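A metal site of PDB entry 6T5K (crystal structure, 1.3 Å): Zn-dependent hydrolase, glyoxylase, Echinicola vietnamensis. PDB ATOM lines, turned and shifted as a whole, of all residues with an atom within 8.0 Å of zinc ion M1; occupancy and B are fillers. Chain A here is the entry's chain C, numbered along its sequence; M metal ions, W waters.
The side-chain amide oxygen of Asn 167 is in hydrogen-bond range of the backbone NH of His 163 (2.9 Å). The side-chain carboxylate (OD2) of Asp 196 lies within hydrogen-bond range of a ring nitrogen (NE2) of His 102, 2.7 Å away. ND1 of His 100 lies close to SG of Cys 105.
Asp 104 touches zinc ion M1 (OD1 to ZN, 3.8 Å). The nearest printed residue that does not touch zinc ion M1 is Cys 182 (4.1 Å).
Zinc ion M1 is bound by water W2 (1.9 Å), NE2 of His 163 (2.0 Å), ND1 of His 102 (2.0 Å) and NE2 of His 100 (2.1 Å). Zinc ion M1 has four donor atoms within binding distance.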
ATOM      1  N   ASP A  71     -15.075  29.459   8.372  1.00  0.00           N
ATOM      2  CA  ASP A  71     -14.208  28.813   9.362  1.00  0.00           C
ATOM      3  C   ASP A  71     -12.738  28.911   8.981  1.00  0.00           C
ATOM      4  O   ASP A  71     -12.360  28.814   7.800  1.00  0.00           O
ATOM      5  CB  ASP A  71     -14.582  27.364   9.630  1.00  0.00           C
ATOM      6  CG  ASP A  71     -15.833  27.215  10.470  1.00  0.00           C
ATOM      7  OD1 ASP A  71     -16.488  28.218  10.794  1.00  0.00           O
ATOM      8  OD2 ASP A  71     -16.162  26.051  10.800  1.00  0.00           O
ATOM      9  N   THR A  99     -18.215  30.236  12.200  1.00  0.00           N
ATOM     10  CA  THR A  99     -19.573  29.739  12.329  1.00  0.00           C
ATOM     11  C   THR A  99     -19.978  29.358  13.763  1.00  0.00           C
ATOM     12  O   THR A  99     -21.159  29.083  13.992  1.00  0.00           O
ATOM     13  CB  THR A  99     -19.875  28.607  11.332  1.00  0.00           C
ATOM     14  OG1 THR A  99     -19.053  27.473  11.571  1.00  0.00           O
ATOM     15  CG2 THR A  99     -19.746  29.103   9.893  1.00  0.00           C
ATOM     16  N   HIS A 100     -19.039  29.310  14.699  1.00  0.00           N
ATOM     17  CA  HIS A 100     -19.338  29.355  16.131  1.00  0.00           C
ATOM     18  C   HIS A 100     -18.028  29.695  16.835  1.00  0.00           C
ATOM     19  O   HIS A 100     -17.000  29.917  16.195  1.00  0.00           O
ATOM     20  CB  HIS A 100     -20.050  28.120  16.714  1.00  0.00           C
ATOM     21  CG  HIS A 100     -19.284  26.836  16.610  1.00  0.00           C
ATOM     22  ND1 HIS A 100     -19.274  26.063  15.472  1.00  0.00           N
ATOM     23  CD2 HIS A 100     -18.579  26.137  17.541  1.00  0.00           C
ATOM     24  CE1 HIS A 100     -18.551  24.979  15.682  1.00  0.00           C
ATOM     25  NE2 HIS A 100     -18.126  24.992  16.932  1.00  0.00           N
ATOM     26  N   PHE A 101     -18.076  29.746  18.157  1.00  0.00           N
ATOM     27  CA  PHE A 101     -16.937  30.294  18.897  1.00  0.00           C
ATOM     28  C   PHE A 101     -15.780  29.323  19.131  1.00  0.00           C
ATOM     29  O   PHE A 101     -14.757  29.750  19.672  1.00  0.00           O
ATOM     30  CB  PHE A 101     -17.399  30.851  20.255  1.00  0.00           C
ATOM     31  CG  PHE A 101     -17.675  29.813  21.312  1.00  0.00           C
ATOM     32  CD1 PHE A 101     -18.935  29.221  21.414  1.00  0.00           C
ATOM     33  CD2 PHE A 101     -16.675  29.453  22.221  1.00  0.00           C
ATOM     34  CE1 PHE A 101     -19.189  28.286  22.399  1.00  0.00           C
ATOM     35  CE2 PHE A 101     -16.947  28.521  23.229  1.00  0.00           C
ATOM     36  CZ  PHE A 101     -18.198  27.918  23.302  1.00  0.00           C
ATOM     37  N   HIS A 102     -15.881  28.059  18.738  1.00  0.00           N
ATOM     38  CA  HIS A 102     -14.822  27.101  19.025  1.00  0.00           C
ATOM     39  C   HIS A 102     -13.595  27.312  18.108  1.00  0.00           C
ATOM     40  O   HIS A 102     -13.649  27.972  17.079  1.00  0.00           O
ATOM     41  CB  HIS A 102     -15.332  25.677  18.830  1.00  0.00           C
ATOM     42  CG  HIS A 102     -16.242  25.189  19.899  1.00  0.00           C
ATOM     43  ND1 HIS A 102     -17.104  24.129  19.714  1.00  0.00           N
ATOM     44  CD2 HIS A 102     -16.423  25.603  21.180  1.00  0.00           C
ATOM     45  CE1 HIS A 102     -17.765  23.897  20.830  1.00  0.00           C
ATOM     46  NE2 HIS A 102     -17.374  24.776  21.738  1.00  0.00           N
ATOM     47  N   LEU A 103     -12.492  26.672  18.483  1.00  0.00           N
ATOM     48  CA  LEU A 103     -11.218  26.916  17.785  1.00  0.00           C
ATOM     49  C   LEU A 103     -11.165  26.347  16.360  1.00  0.00           C
ATOM     50  O   LEU A 103     -10.407  26.860  15.530  1.00  0.00           O
ATOM     51  CB  LEU A 103     -10.057  26.427  18.645  1.00  0.00           C
ATOM     52  CG  LEU A 103      -9.823  27.277  19.902  1.00  0.00           C
ATOM     53  CD1 LEU A 103      -8.798  26.565  20.778  1.00  0.00           C
ATOM     54  CD2 LEU A 103      -9.308  28.675  19.559  1.00  0.00           C
ATOM     55  N   ASP A 104     -11.974  25.341  16.039  1.00  0.00           N
ATOM     56  CA  ASP A 104     -12.034  24.848  14.668  1.00  0.00           C
ATOM     57  C   ASP A 104     -12.918  25.726  13.770  1.00  0.00           C
ATOM     58  O   ASP A 104     -13.250  25.332  12.642  1.00  0.00           O
ATOM     59  CB  ASP A 104     -12.467  23.370  14.595  1.00  0.00           C
ATOM     60  CG  ASP A 104     -13.818  23.077  15.269  1.00  0.00           C
ATOM     61  OD1 ASP A 104     -14.061  23.637  16.377  1.00  0.00           O
ATOM     62  OD2 ASP A 104     -14.605  22.232  14.710  1.00  0.00           O
ATOM     63  N   CYS A 105     -13.310  26.886  14.289  1.00  0.00           N
ATOM     64  CA  CYS A 105     -13.957  27.931  13.526  1.00  0.00           C
ATOM     65  C   CYS A 105     -13.127  29.195  13.489  1.00  0.00           C
ATOM     66  O   CYS A 105     -13.175  29.923  12.495  1.00  0.00           O
ATOM     67  CB  CYS A 105     -15.321  28.271  14.142  1.00  0.00           C
ATOM     68  SG  CYS A 105     -16.374  26.850  14.308  1.00  0.00           S
ATOM     69  N   HIS A 163     -25.158  22.422  18.175  1.00  0.00           N
ATOM     70  CA  HIS A 163     -23.794  22.104  18.581  1.00  0.00           C
ATOM     71  C   HIS A 163     -23.275  23.112  19.602  1.00  0.00           C
ATOM     72  O   HIS A 163     -22.622  22.746  20.581  1.00  0.00           O
ATOM     73  CB  HIS A 163     -22.897  22.113  17.350  1.00  0.00           C
ATOM     74  CG  HIS A 163     -21.453  22.012  17.667  1.00  0.00           C
ATOM     75  ND1 HIS A 163     -20.860  20.859  18.156  1.00  0.00           N
ATOM     76  CD2 HIS A 163     -20.468  22.930  17.606  1.00  0.00           C
ATOM     77  CE1 HIS A 163     -19.573  21.075  18.353  1.00  0.00           C
ATOM     78  NE2 HIS A 163     -19.313  22.325  18.030  1.00  0.00           N
ATOM     79  N   THR A 164     -23.593  24.379  19.395  1.00  0.00           N
ATOM     80  CA  THR A 164     -23.391  25.414  20.407  1.00  0.00           C
ATOM     81  C   THR A 164     -24.596  26.353  20.382  1.00  0.00           C
ATOM     82  O   THR A 164     -25.481  26.249  19.520  1.00  0.00           O
ATOM     83  CB  THR A 164     -22.120  26.249  20.168  1.00  0.00           C
ATOM     84  OG1 THR A 164     -22.200  26.832  18.864  1.00  0.00           O
ATOM     85  CG2 THR A 164     -20.864  25.410  20.318  1.00  0.00           C
ATOM     86  N   ASP A 166     -24.496  29.476  19.647  1.00  0.00           N
ATOM     87  CA  ASP A 166     -24.253  30.543  18.697  1.00  0.00           C
ATOM     88  C   ASP A 166     -24.058  30.053  17.257  1.00  0.00           C
ATOM     89  O   ASP A 166     -23.730  30.870  16.397  1.00  0.00           O
ATOM     90  CB  ASP A 166     -23.018  31.338  19.128  1.00  0.00           C
ATOM     91  CG  ASP A 166     -21.756  30.465  19.188  1.00  0.00           C
ATOM     92  OD1 ASP A 166     -21.822  29.314  19.650  1.00  0.00           O
ATOM     93  OD2 ASP A 166     -20.679  30.984  18.769  1.00  0.00           O
ATOM     94  N   ASN A 167     -24.172  28.765  17.027  1.00  0.00           N
ATOM     95  CA  ASN A 167     -23.834  28.271  15.709  1.00  0.00           C
ATOM     96  C   ASN A 167     -24.683  28.805  14.564  1.00  0.00           C
ATOM     97  O   ASN A 167     -25.846  28.953  14.715  1.00  0.00           O
ATOM     98  CB  ASN A 167     -23.671  26.740  15.679  1.00  0.00           C
ATOM     99  CG  ASN A 167     -24.869  25.973  16.253  1.00  0.00           C
ATOM    100  OD1 ASN A 167     -24.752  24.847  16.642  1.00  0.00           O
ATOM    101  ND2 ASN A 167     -25.957  26.568  16.215  1.00  0.00           N
ATOM    102  N   GLY A 181     -21.410  23.526   9.157  1.00  0.00           N
ATOM    103  CA  GLY A 181     -20.534  23.579  10.308  1.00  0.00           C
ATOM    104  C   GLY A 181     -20.850  22.448  11.261  1.00  0.00           C
ATOM    105  O   GLY A 181     -21.443  21.435  10.867  1.00  0.00           O
ATOM    106  N   CYS A 182     -20.471  22.632  12.537  1.00  0.00           N
ATOM    107  CA  CYS A 182     -20.550  21.514  13.453  1.00  0.00           C
ATOM    108  C   CYS A 182     -21.961  21.215  13.910  1.00  0.00           C
ATOM    109  O   CYS A 182     -22.173  20.219  14.608  1.00  0.00           O
ATOM    110  CB  CYS A 182     -19.615  21.687  14.608  1.00  0.00           C
ATOM    111  SG  CYS A 182     -17.932  21.969  14.022  1.00  0.00           S
ATOM    112  N   LEU A 183     -22.916  22.071  13.525  1.00  0.00           N
ATOM    113  CA  LEU A 183     -24.331  21.801  13.750  1.00  0.00           C
ATOM    114  C   LEU A 183     -24.818  20.643  12.905  1.00  0.00           C
ATOM    115  O   LEU A 183     -25.817  20.009  13.264  1.00  0.00           O
ATOM    116  CB  LEU A 183     -25.118  23.060  13.369  1.00  0.00           C
ATOM    117  CG  LEU A 183     -26.633  23.129  13.455  1.00  0.00           C
ATOM    118  CD1 LEU A 183     -27.083  22.968  14.863  1.00  0.00           C
ATOM    119  CD2 LEU A 183     -27.045  24.455  12.835  1.00  0.00           C
ATOM    120  N   LYS A 185     -23.995  16.965  11.123  1.00  0.00           N
ATOM    121  CA  LYS A 185     -23.147  15.783  11.156  1.00  0.00           C
ATOM    122  C   LYS A 185     -23.066  15.103   9.797  1.00  0.00           C
ATOM    123  O   LYS A 185     -24.010  15.136   9.003  1.00  0.00           O
ATOM    124  CB  LYS A 185     -23.661  14.755  12.166  1.00  0.00           C
ATOM    125  CG  LYS A 185     -23.767  15.309  13.552  1.00  0.00           C
ATOM    126  CD  LYS A 185     -22.434  15.821  14.048  1.00  0.00           C
ATOM    127  CE  LYS A 185     -22.484  16.147  15.558  1.00  0.00           C
ATOM    128  NZ  LYS A 185     -21.205  16.616  16.078  1.00  0.00           N
ATOM    129  N   ASN A 193     -18.706  16.166  20.153  1.00  0.00           N
ATOM    130  CA  ASN A 193     -18.503  16.909  21.382  1.00  0.00           C
ATOM    131  C   ASN A 193     -19.789  17.623  21.752  1.00  0.00           C
ATOM    132  O   ASN A 193     -20.236  18.534  21.035  1.00  0.00           O
ATOM    133  CB  ASN A 193     -17.379  17.912  21.172  1.00  0.00           C
ATOM    134  CG  ASN A 193     -17.295  18.912  22.279  1.00  0.00           C
ATOM    135  OD1 ASN A 193     -17.674  18.612  23.425  1.00  0.00           O
ATOM    136  ND2 ASN A 193     -16.808  20.119  21.965  1.00  0.00           N
ATOM    137  N   ASP A 196     -20.780  21.844  24.890  1.00  0.00           N
ATOM    138  CA  ASP A 196     -21.388  23.167  24.767  1.00  0.00           C
ATOM    139  C   ASP A 196     -22.732  23.105  24.026  1.00  0.00           C
ATOM    140  O   ASP A 196     -23.274  24.140  23.622  1.00  0.00           O
ATOM    141  CB  ASP A 196     -20.435  24.135  24.079  1.00  0.00           C
ATOM    142  CG  ASP A 196     -19.199  24.426  24.915  1.00  0.00           C
ATOM    143  OD1 ASP A 196     -19.363  24.567  26.164  1.00  0.00           O
ATOM    144  OD2 ASP A 196     -18.085  24.553  24.315  1.00  0.00           O
ATOM    145  N   HIS A 223     -17.316  18.222  10.321  1.00  0.00           N
ATOM    146  CA  HIS A 223     -16.347  17.143  10.372  1.00  0.00           C
ATOM    147  C   HIS A 223     -16.861  16.022   9.484  1.00  0.00           C
ATOM    148  O   HIS A 223     -18.071  15.783   9.448  1.00  0.00           O
ATOM    149  CB  HIS A 223     -16.191  16.645  11.825  1.00  0.00           C
ATOM    150  CG  HIS A 223     -15.848  17.740  12.800  1.00  0.00           C
ATOM    151  ND1 HIS A 223     -14.567  18.205  12.998  1.00  0.00           N
ATOM    152  CD2 HIS A 223     -16.646  18.504  13.596  1.00  0.00           C
ATOM    153  CE1 HIS A 223     -14.584  19.196  13.878  1.00  0.00           C
ATOM    154  NE2 HIS A 223     -15.831  19.383  14.269  1.00  0.00           N
HETATM  155 ZN    ZN M   1     -17.548  23.276  17.915  1.00  0.00          ZN
HETATM  156 ZN    ZN M   2     -16.531  21.150  15.350  1.00  0.00          ZN
HETATM  157  O   HOH W   1     -16.165  20.785  19.162  1.00  0.00           O
HETATM  158  O   HOH W   2     -16.154  22.247  17.142  1.00  0.00           O
